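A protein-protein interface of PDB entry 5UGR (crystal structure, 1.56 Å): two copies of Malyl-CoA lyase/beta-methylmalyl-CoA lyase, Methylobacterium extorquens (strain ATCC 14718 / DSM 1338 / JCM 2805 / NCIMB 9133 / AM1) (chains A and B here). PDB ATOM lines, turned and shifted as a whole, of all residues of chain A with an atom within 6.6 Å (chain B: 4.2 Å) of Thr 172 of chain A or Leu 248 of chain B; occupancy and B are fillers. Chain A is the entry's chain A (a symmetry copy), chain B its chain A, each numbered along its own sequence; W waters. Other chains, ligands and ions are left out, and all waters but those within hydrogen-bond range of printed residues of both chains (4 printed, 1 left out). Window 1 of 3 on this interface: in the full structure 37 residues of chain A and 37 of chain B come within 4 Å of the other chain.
The backbone carbonyl oxygen of Ala 247 of chain B sits at hydrogen-bond distance from the backbone NH of Arg 175 of chain A.
O of Thr 172 of chain A sits at hydrogen-bond distance from NE of Arg 218 of chain B (3.0 Å).
OH of Tyr 186 of chain A lies within hydrogen-bond range of ND2 of Asn 211 of chain B, at 3.4 Å.
NH2 of Arg 218 of chain B lies close to NH1 of Arg 173 of chain A (3.5 Å).
O of Arg 175 of chain A sits close to OD1 of Asn 183 of chain A (3.3 Å).
O of Ala 169 of chain A sits at hydrogen-bond distance from OG1 of Thr 172 of chain A (3.3 Å).
O of Tyr 168 of chain A is in hydrogen-bond range of OG1 of Thr 172 of chain A, at 3.0 Å.
The side-chain hydroxyl (OG) of Ser 171 of chain A lies within hydrogen-bond range of the backbone NH (N) of Ala 142 of chain A.
The guanidinium group (NH2) of Arg 218 of chain B lies within hydrogen-bond range of the backbone carbonyl oxygen (O) of Gly 249 of chain B (2.7 Å).
O of Ala 169 of chain A sits at hydrogen-bond distance from N of Ala 174 of chain A (2.9 Å).
Ala 142 of chain A touches Arg 218 of chain B.
O of Ser 171 of chain A touches CB of Arg 218 of chain B, at 3.8 Å.
Leu 248 of chain B touches Thr 172 of chain A.
O of Arg 173 of chain A touches CA of Gly 249 of chain B, 3.4 Å away.
Ala 174 of chain A touches Leu 248 of chain B (CA to O, 3.6 Å).
Gly 249 of chain B touches Ala 174 of chain A (N to CA, 3.9 Å).
Ala 246 of chain B touches Arg 175 of chain A.
Ala 247 of chain B touches Asn 183 of chain A (CB to OD1, 3.7 Å).
Tyr 186 of chain A touches Arg 244 of chain B.
Tyr 186 of chain A touches Leu 248 of chain B (CE1 to CD2, 3.3 Å).
Of the printed residues of chain B, Ser 171 of chain A touches Arg 218.
Of the printed residues of chain B, Thr 172 of chain A touches Arg 218 (3.0 Å), Leu 248 (3.7 Å) and Gly 249 (3.3 Å).
Asp 204 of chain A touches none of the printed residues of chain B.
Leu 248 of chain B touches three residues of chain A.
Printed residues of chain A within 4 Å of Gly 249 of chain B: Thr 172, Arg 173 and Ala 174.
The nearest residue of chain B that does not touch Thr 172 of chain A is Leu 214 of chain B (4.1 Å).
The nearest printed residue of chain B that does not touch Tyr 186 of chain A is Ala 247 of chain B (4.2 Å).
Along chain A the printed residues that touch a printed residue of chain B span positions 142 to 186.
Printed residues of chain B that touch a printed residue of chain A: Asn 211, Arg 218, Arg 244, Ala 246, Ala 247, Leu 248 and Gly 249.
Hydrophobic or aromatic side chains of chain B that line the printed part of chain A: Ala 246, Ala 247 and Leu 248.
Among the printed residues, 16 pairs touch across the chains.
No position is printed for both chains.
Water W2 bridges the side-chain hydroxyl (OH) of Tyr 168 of chain A (2.7 Å) and the side-chain amide oxygen (OD1) of Asn 211 of chain B (2.8 Å).
Water W4 bridges the backbone carbonyl oxygen of Ser 171 of chain A (2.7 Å) and the backbone carbonyl oxygen of Arg 218 of chain B (2.9 Å).
Water W1 bridges O of Leu 248 of chain B (2.8 Å) and OG1 of Thr 172 of chain A (2.9 Å).
Water W3 lies within hydrogen-bond range of O of Pro 205 of chain A and OD1 of Asn 211 of chain B.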
ATOM      1  N   THR A 141      17.922   1.378 -17.550  1.00  0.00           N
ATOM      2  CA  THR A 141      18.467   1.308 -16.211  1.00  0.00           C
ATOM      3  C   THR A 141      17.814   2.422 -15.402  1.00  0.00           C
ATOM      4  O   THR A 141      17.302   3.426 -15.974  1.00  0.00           O
ATOM      5  CB  THR A 141      20.001   1.544 -16.179  1.00  0.00           C
ATOM      6  OG1 THR A 141      20.295   2.869 -16.656  1.00  0.00           O
ATOM      7  CG2 THR A 141      20.760   0.512 -16.983  1.00  0.00           C
ATOM      8  N   ALA A 142      17.817   2.275 -14.078  1.00  0.00           N
ATOM      9  CA  ALA A 142      17.351   3.371 -13.216  1.00  0.00           C
ATOM     10  C   ALA A 142      18.173   4.616 -13.357  1.00  0.00           C
ATOM     11  O   ALA A 142      17.635   5.721 -13.335  1.00  0.00           O
ATOM     12  CB  ALA A 142      17.344   2.895 -11.780  1.00  0.00           C
ATOM     13  N   ASP A 167      15.513  -4.982 -18.899  1.00  0.00           N
ATOM     14  CA  ASP A 167      16.721  -4.478 -18.226  1.00  0.00           C
ATOM     15  C   ASP A 167      16.406  -3.396 -17.201  1.00  0.00           C
ATOM     16  O   ASP A 167      17.052  -3.315 -16.133  1.00  0.00           O
ATOM     17  CB  ASP A 167      17.868  -4.180 -19.194  1.00  0.00           C
ATOM     18  CG  ASP A 167      18.532  -5.470 -19.707  1.00  0.00           C
ATOM     19  OD1 ASP A 167      18.398  -6.515 -19.052  1.00  0.00           O
ATOM     20  OD2 ASP A 167      19.257  -5.396 -20.709  1.00  0.00           O
ATOM     21  N   TYR A 168      15.366  -2.604 -17.486  1.00  0.00           N
ATOM     22  CA  TYR A 168      14.917  -1.641 -16.500  1.00  0.00           C
ATOM     23  C   TYR A 168      14.380  -2.340 -15.248  1.00  0.00           C
ATOM     24  O   TYR A 168      14.700  -1.941 -14.109  1.00  0.00           O
ATOM     25  CB  TYR A 168      13.856  -0.713 -17.093  1.00  0.00           C
ATOM     26  CG  TYR A 168      13.235   0.237 -16.131  1.00  0.00           C
ATOM     27  CD1 TYR A 168      13.857   1.416 -15.808  1.00  0.00           C
ATOM     28  CD2 TYR A 168      12.017  -0.043 -15.548  1.00  0.00           C
ATOM     29  CE1 TYR A 168      13.277   2.319 -14.939  1.00  0.00           C
ATOM     30  CE2 TYR A 168      11.419   0.854 -14.645  1.00  0.00           C
ATOM     31  CZ  TYR A 168      12.059   2.027 -14.347  1.00  0.00           C
ATOM     32  OH  TYR A 168      11.493   2.945 -13.497  1.00  0.00           O
ATOM     33  N   ALA A 169      13.569  -3.374 -15.456  1.00  0.00           N
ATOM     34  CA  ALA A 169      13.079  -4.175 -14.328  1.00  0.00           C
ATOM     35  C   ALA A 169      14.236  -4.719 -13.503  1.00  0.00           C
ATOM     36  O   ALA A 169      14.219  -4.675 -12.292  1.00  0.00           O
ATOM     37  CB  ALA A 169      12.181  -5.280 -14.865  1.00  0.00           C
ATOM     38  N   ALA A 170      15.263  -5.251 -14.189  1.00  0.00           N
ATOM     39  CA  ALA A 170      16.406  -5.797 -13.455  1.00  0.00           C
ATOM     40  C   ALA A 170      17.114  -4.727 -12.621  1.00  0.00           C
ATOM     41  O   ALA A 170      17.478  -4.927 -11.471  1.00  0.00           O
ATOM     42  CB  ALA A 170      17.374  -6.474 -14.409  1.00  0.00           C
ATOM     43  N   SER A 171      17.277  -3.553 -13.215  1.00  0.00           N
ATOM     44  CA  SER A 171      17.957  -2.435 -12.574  1.00  0.00           C
ATOM     45  C   SER A 171      17.182  -1.933 -11.346  1.00  0.00           C
ATOM     46  O   SER A 171      17.776  -1.501 -10.358  1.00  0.00           O
ATOM     47  CB  SER A 171      18.151  -1.275 -13.585  1.00  0.00           C
ATOM     48  OG  SER A 171      18.834  -0.189 -13.020  1.00  0.00           O
ATOM     49  N   THR A 172      15.856  -1.950 -11.440  1.00  0.00           N
ATOM     50  CA  THR A 172      15.024  -1.461 -10.333  1.00  0.00           C
ATOM     51  C   THR A 172      14.714  -2.551  -9.295  1.00  0.00           C
ATOM     52  O   THR A 172      14.145  -2.279  -8.225  1.00  0.00           O
ATOM     53  CB  THR A 172      13.709  -0.812 -10.819  1.00  0.00           C
ATOM     54  OG1 THR A 172      12.978  -1.709 -11.660  1.00  0.00           O
ATOM     55  CG2 THR A 172      13.958   0.533 -11.541  1.00  0.00           C
ATOM     56  N   ARG A 173      15.117  -3.785  -9.593  1.00  0.00           N
ATOM     57  CA  ARG A 173      14.808  -5.017  -8.797  1.00  0.00           C
ATOM     58  C   ARG A 173      13.288  -5.317  -8.808  1.00  0.00           C
ATOM     59  O   ARG A 173      12.755  -5.965  -7.878  1.00  0.00           O
ATOM     60  CB  ARG A 173      15.423  -4.970  -7.370  1.00  0.00           C
ATOM     61  CG  ARG A 173      16.186  -6.208  -6.975  1.00  0.00           C
ATOM     62  CD  ARG A 173      16.721  -6.236  -5.544  1.00  0.00           C
ATOM     63  NE  ARG A 173      15.834  -6.774  -4.425  1.00  0.00           N
ATOM     64  CZ  ARG A 173      15.954  -6.454  -3.119  1.00  0.00           C
ATOM     65  NH1 ARG A 173      16.853  -5.539  -2.715  1.00  0.00           N
ATOM     66  NH2 ARG A 173      15.134  -7.002  -2.186  1.00  0.00           N
ATOM     67  N   ALA A 174      12.570  -4.881  -9.855  1.00  0.00           N
ATOM     68  CA  ALA A 174      11.207  -5.221 -10.040  1.00  0.00           C
ATOM     69  C   ALA A 174      11.066  -6.715 -10.098  1.00  0.00           C
ATOM     70  O   ALA A 174      11.957  -7.445 -10.638  1.00  0.00           O
ATOM     71  CB  ALA A 174      10.653  -4.559 -11.280  1.00  0.00           C
ATOM     72  N   ARG A 175       9.919  -7.202  -9.594  1.00  0.00           N
ATOM     73  CA  ARG A 175       9.694  -8.657  -9.583  1.00  0.00           C
ATOM     74  C   ARG A 175       9.197  -8.979 -10.963  1.00  0.00           C
ATOM     75  O   ARG A 175       8.100  -8.600 -11.344  1.00  0.00           O
ATOM     76  CB  ARG A 175       8.751  -9.049  -8.460  1.00  0.00           C
ATOM     77  CG  ARG A 175       9.408  -8.849  -7.087  1.00  0.00           C
ATOM     78  CD  ARG A 175       8.488  -9.174  -5.936  1.00  0.00           C
ATOM     79  NE  ARG A 175       9.289  -9.386  -4.748  1.00  0.00           N
ATOM     80  CZ  ARG A 175       8.813  -9.763  -3.565  1.00  0.00           C
ATOM     81  NH1 ARG A 175       7.469  -9.863  -3.330  1.00  0.00           N
ATOM     82  NH2 ARG A 175       9.697 -10.024  -2.609  1.00  0.00           N
ATOM     83  N   ASN A 183       1.517  -7.840 -13.719  1.00  0.00           N
ATOM     84  CA  ASN A 183       1.808  -8.553 -12.483  1.00  0.00           C
ATOM     85  C   ASN A 183       0.617  -8.506 -11.548  1.00  0.00           C
ATOM     86  O   ASN A 183       0.177  -7.389 -11.179  1.00  0.00           O
ATOM     87  CB  ASN A 183       3.025  -7.860 -11.838  1.00  0.00           C
ATOM     88  CG  ASN A 183       3.623  -8.603 -10.668  1.00  0.00           C
ATOM     89  OD1 ASN A 183       4.881  -8.547 -10.419  1.00  0.00           O
ATOM     90  ND2 ASN A 183       2.835  -9.307  -9.976  1.00  0.00           N
ATOM     91  N   TYR A 186       0.908  -6.193  -8.716  1.00  0.00           N
ATOM     92  CA  TYR A 186       0.960  -4.733  -8.926  1.00  0.00           C
ATOM     93  C   TYR A 186      -0.498  -4.324  -9.209  1.00  0.00           C
ATOM     94  O   TYR A 186      -0.964  -4.192 -10.360  1.00  0.00           O
ATOM     95  CB  TYR A 186       1.924  -4.322 -10.036  1.00  0.00           C
ATOM     96  CG  TYR A 186       2.239  -2.849  -9.934  1.00  0.00           C
ATOM     97  CD1 TYR A 186       2.878  -2.339  -8.834  1.00  0.00           C
ATOM     98  CD2 TYR A 186       1.820  -1.935 -10.896  1.00  0.00           C
ATOM     99  CE1 TYR A 186       3.102  -0.994  -8.646  1.00  0.00           C
ATOM    100  CE2 TYR A 186       2.027  -0.584 -10.726  1.00  0.00           C
ATOM    101  CZ  TYR A 186       2.685  -0.097  -9.606  1.00  0.00           C
ATOM    102  OH  TYR A 186       2.935   1.244  -9.430  1.00  0.00           O
ATOM    103  N   ASP A 204      -0.452  -0.557 -13.835  1.00  0.00           N
ATOM    104  CA  ASP A 204       0.556  -0.670 -14.901  1.00  0.00           C
ATOM    105  C   ASP A 204       1.932  -0.464 -14.285  1.00  0.00           C
ATOM    106  O   ASP A 204       2.305   0.661 -13.985  1.00  0.00           O
ATOM    107  CB  ASP A 204       0.264   0.375 -15.969  1.00  0.00           C
ATOM    108  CG  ASP A 204       1.222   0.348 -17.137  1.00  0.00           C
ATOM    109  OD1 ASP A 204       2.233  -0.364 -17.093  1.00  0.00           O
ATOM    110  OD2 ASP A 204       0.933   1.090 -18.105  1.00  0.00           O
ATOM    111  N   PRO A 205       2.754  -1.536 -14.195  1.00  0.00           N
ATOM    112  CA  PRO A 205       4.060  -1.404 -13.545  1.00  0.00           C
ATOM    113  C   PRO A 205       5.037  -0.515 -14.292  1.00  0.00           C
ATOM    114  O   PRO A 205       6.040  -0.092 -13.716  1.00  0.00           O
ATOM    115  CB  PRO A 205       4.599  -2.829 -13.497  1.00  0.00           C
ATOM    116  CG  PRO A 205       3.766  -3.587 -14.399  1.00  0.00           C
ATOM    117  CD  PRO A 205       2.502  -2.880 -14.701  1.00  0.00           C
ATOM    118  N   TRP A 206       4.761  -0.254 -15.566  1.00  0.00           N
ATOM    119  CA  TRP A 206       5.656   0.535 -16.407  1.00  0.00           C
ATOM    120  C   TRP A 206       5.125   1.933 -16.706  1.00  0.00           C
ATOM    121  O   TRP A 206       5.749   2.662 -17.486  1.00  0.00           O
ATOM    122  CB  TRP A 206       6.009  -0.223 -17.707  1.00  0.00           C
ATOM    123  CG  TRP A 206       6.208  -1.691 -17.505  1.00  0.00           C
ATOM    124  CD1 TRP A 206       5.416  -2.701 -18.004  1.00  0.00           C
ATOM    125  CD2 TRP A 206       7.163  -2.318 -16.627  1.00  0.00           C
ATOM    126  NE1 TRP A 206       5.874  -3.903 -17.541  1.00  0.00           N
ATOM    127  CE2 TRP A 206       6.935  -3.703 -16.688  1.00  0.00           C
ATOM    128  CE3 TRP A 206       8.228  -1.851 -15.869  1.00  0.00           C
ATOM    129  CZ2 TRP A 206       7.684  -4.610 -15.928  1.00  0.00           C
ATOM    130  CZ3 TRP A 206       8.950  -2.767 -15.112  1.00  0.00           C
ATOM    131  CH2 TRP A 206       8.666  -4.112 -15.154  1.00  0.00           C
ATOM    132  N   ASN B 211       7.152   5.373  -7.467  1.00  0.00           N
ATOM    133  CA  ASN B 211       8.012   5.116  -8.597  1.00  0.00           C
ATOM    134  C   ASN B 211       9.119   6.158  -8.665  1.00  0.00           C
ATOM    135  O   ASN B 211      10.261   5.837  -8.978  1.00  0.00           O
ATOM    136  CB  ASN B 211       7.257   5.077  -9.914  1.00  0.00           C
ATOM    137  CG  ASN B 211       6.581   3.708 -10.199  1.00  0.00           C
ATOM    138  OD1 ASN B 211       7.159   2.831 -10.858  1.00  0.00           O
ATOM    139  ND2 ASN B 211       5.375   3.529  -9.691  1.00  0.00           N
ATOM    140  N   LEU B 214      11.589   5.339  -5.978  1.00  0.00           N
ATOM    141  CA  LEU B 214      12.257   4.098  -6.381  1.00  0.00           C
ATOM    142  C   LEU B 214      13.372   4.350  -7.393  1.00  0.00           C
ATOM    143  O   LEU B 214      14.491   3.837  -7.258  1.00  0.00           O
ATOM    144  CB  LEU B 214      11.243   3.131  -6.953  1.00  0.00           C
ATOM    145  CG  LEU B 214      11.799   1.844  -7.611  1.00  0.00           C
ATOM    146  CD1 LEU B 214      12.062   0.814  -6.579  1.00  0.00           C
ATOM    147  CD2 LEU B 214      10.921   1.380  -8.709  1.00  0.00           C
ATOM    148  N   ARG B 218      17.255   3.473  -6.862  1.00  0.00           N
ATOM    149  CA  ARG B 218      17.884   2.414  -7.681  1.00  0.00           C
ATOM    150  C   ARG B 218      18.955   2.981  -8.618  1.00  0.00           C
ATOM    151  O   ARG B 218      19.896   2.273  -8.984  1.00  0.00           O
ATOM    152  CB  ARG B 218      16.821   1.577  -8.410  1.00  0.00           C
ATOM    153  CG  ARG B 218      15.973   0.769  -7.462  1.00  0.00           C
ATOM    154  CD  ARG B 218      16.759  -0.357  -6.858  1.00  0.00           C
ATOM    155  NE  ARG B 218      15.926  -1.279  -6.074  1.00  0.00           N
ATOM    156  CZ  ARG B 218      16.364  -1.962  -5.007  1.00  0.00           C
ATOM    157  NH1 ARG B 218      17.584  -1.784  -4.543  1.00  0.00           N
ATOM    158  NH2 ARG B 218      15.551  -2.769  -4.374  1.00  0.00           N
ATOM    159  N   ARG B 244       2.435  -4.827  -3.658  1.00  0.00           N
ATOM    160  CA  ARG B 244       2.401  -3.893  -4.780  1.00  0.00           C
ATOM    161  C   ARG B 244       3.740  -3.124  -4.879  1.00  0.00           C
ATOM    162  O   ARG B 244       4.385  -3.091  -5.946  1.00  0.00           O
ATOM    163  CB  ARG B 244       1.211  -2.929  -4.678  1.00  0.00           C
ATOM    164  CG  ARG B 244       1.212  -1.887  -5.748  1.00  0.00           C
ATOM    165  CD  ARG B 244      -0.037  -1.008  -5.838  1.00  0.00           C
ATOM    166  NE  ARG B 244      -0.241  -0.164  -4.677  1.00  0.00           N
ATOM    167  CZ  ARG B 244      -1.062  -0.417  -3.660  1.00  0.00           C
ATOM    168  NH1 ARG B 244      -1.837  -1.501  -3.613  1.00  0.00           N
ATOM    169  NH2 ARG B 244      -1.152   0.462  -2.686  1.00  0.00           N
ATOM    170  N   CYS B 245       4.237  -2.567  -3.767  1.00  0.00           N
ATOM    171  CA  CYS B 245       5.513  -1.876  -3.874  1.00  0.00           C
ATOM    172  C   CYS B 245       6.664  -2.848  -4.046  1.00  0.00           C
ATOM    173  O   CYS B 245       7.643  -2.515  -4.710  1.00  0.00           O
ATOM    174  CB  CYS B 245       5.715  -0.919  -2.743  1.00  0.00           C
ATOM    175  SG  CYS B 245       6.051  -1.579  -1.142  1.00  0.00           S
ATOM    176  N   ALA B 246       6.574  -4.036  -3.467  1.00  0.00           N
ATOM    177  CA  ALA B 246       7.635  -5.045  -3.709  1.00  0.00           C
ATOM    178  C   ALA B 246       7.739  -5.365  -5.188  1.00  0.00           C
ATOM    179  O   ALA B 246       8.860  -5.591  -5.704  1.00  0.00           O
ATOM    180  CB  ALA B 246       7.351  -6.297  -2.908  1.00  0.00           C
ATOM    181  N   ALA B 247       6.593  -5.425  -5.883  1.00  0.00           N
ATOM    182  CA  ALA B 247       6.599  -5.735  -7.315  1.00  0.00           C
ATOM    183  C   ALA B 247       7.392  -4.711  -8.107  1.00  0.00           C
ATOM    184  O   ALA B 247       8.001  -5.050  -9.114  1.00  0.00           O
ATOM    185  CB  ALA B 247       5.196  -5.859  -7.852  1.00  0.00           C
ATOM    186  N   LEU B 248       7.344  -3.464  -7.673  1.00  0.00           N
ATOM    187  CA  LEU B 248       8.157  -2.394  -8.304  1.00  0.00           C
ATOM    188  C   LEU B 248       9.647  -2.498  -8.066  1.00  0.00           C
ATOM    189  O   LEU B 248      10.460  -1.886  -8.778  1.00  0.00           O
ATOM    190  CB  LEU B 248       7.782  -1.055  -7.778  1.00  0.00           C
ATOM    191  CG  LEU B 248       6.465  -0.511  -8.044  1.00  0.00           C
ATOM    192  CD1 LEU B 248       6.288   0.839  -7.317  1.00  0.00           C
ATOM    193  CD2 LEU B 248       6.233  -0.353  -9.570  1.00  0.00           C
ATOM    194  N   GLY B 249      10.015  -3.150  -6.959  1.00  0.00           N
ATOM    195  CA  GLY B 249      11.411  -3.165  -6.532  1.00  0.00           C
ATOM    196  C   GLY B 249      11.686  -2.613  -5.150  1.00  0.00           C
ATOM    197  O   GLY B 249      12.866  -2.462  -4.793  1.00  0.00           O
ATOM    198  N   PHE B 250      10.651  -2.228  -4.395  1.00  0.00           N
ATOM    199  CA  PHE B 250      10.914  -1.813  -3.012  1.00  0.00           C
ATOM    200  C   PHE B 250      11.441  -2.999  -2.199  1.00  0.00           C
ATOM    201  O   PHE B 250      11.093  -4.159  -2.468  1.00  0.00           O
ATOM    202  CB  PHE B 250       9.651  -1.302  -2.329  1.00  0.00           C
ATOM    203  CG  PHE B 250       9.293   0.139  -2.636  1.00  0.00           C
ATOM    204  CD1 PHE B 250       8.998   0.563  -3.939  1.00  0.00           C
ATOM    205  CD2 PHE B 250       9.376   1.084  -1.645  1.00  0.00           C
ATOM    206  CE1 PHE B 250       8.730   1.906  -4.219  1.00  0.00           C
ATOM    207  CE2 PHE B 250       9.096   2.406  -1.910  1.00  0.00           C
ATOM    208  CZ  PHE B 250       8.778   2.822  -3.206  1.00  0.00           C
HETATM  209  O   HOH W   1      10.284  -0.781 -11.328  1.00  0.00           O
HETATM  210  O   HOH W   2       9.456   1.843 -12.057  1.00  0.00           O
HETATM  211  O   HOH W   3       7.500   2.328 -14.155  1.00  0.00           O
HETATM  212  O   HOH W   4      20.041  -0.589  -9.113  1.00  0.00           O
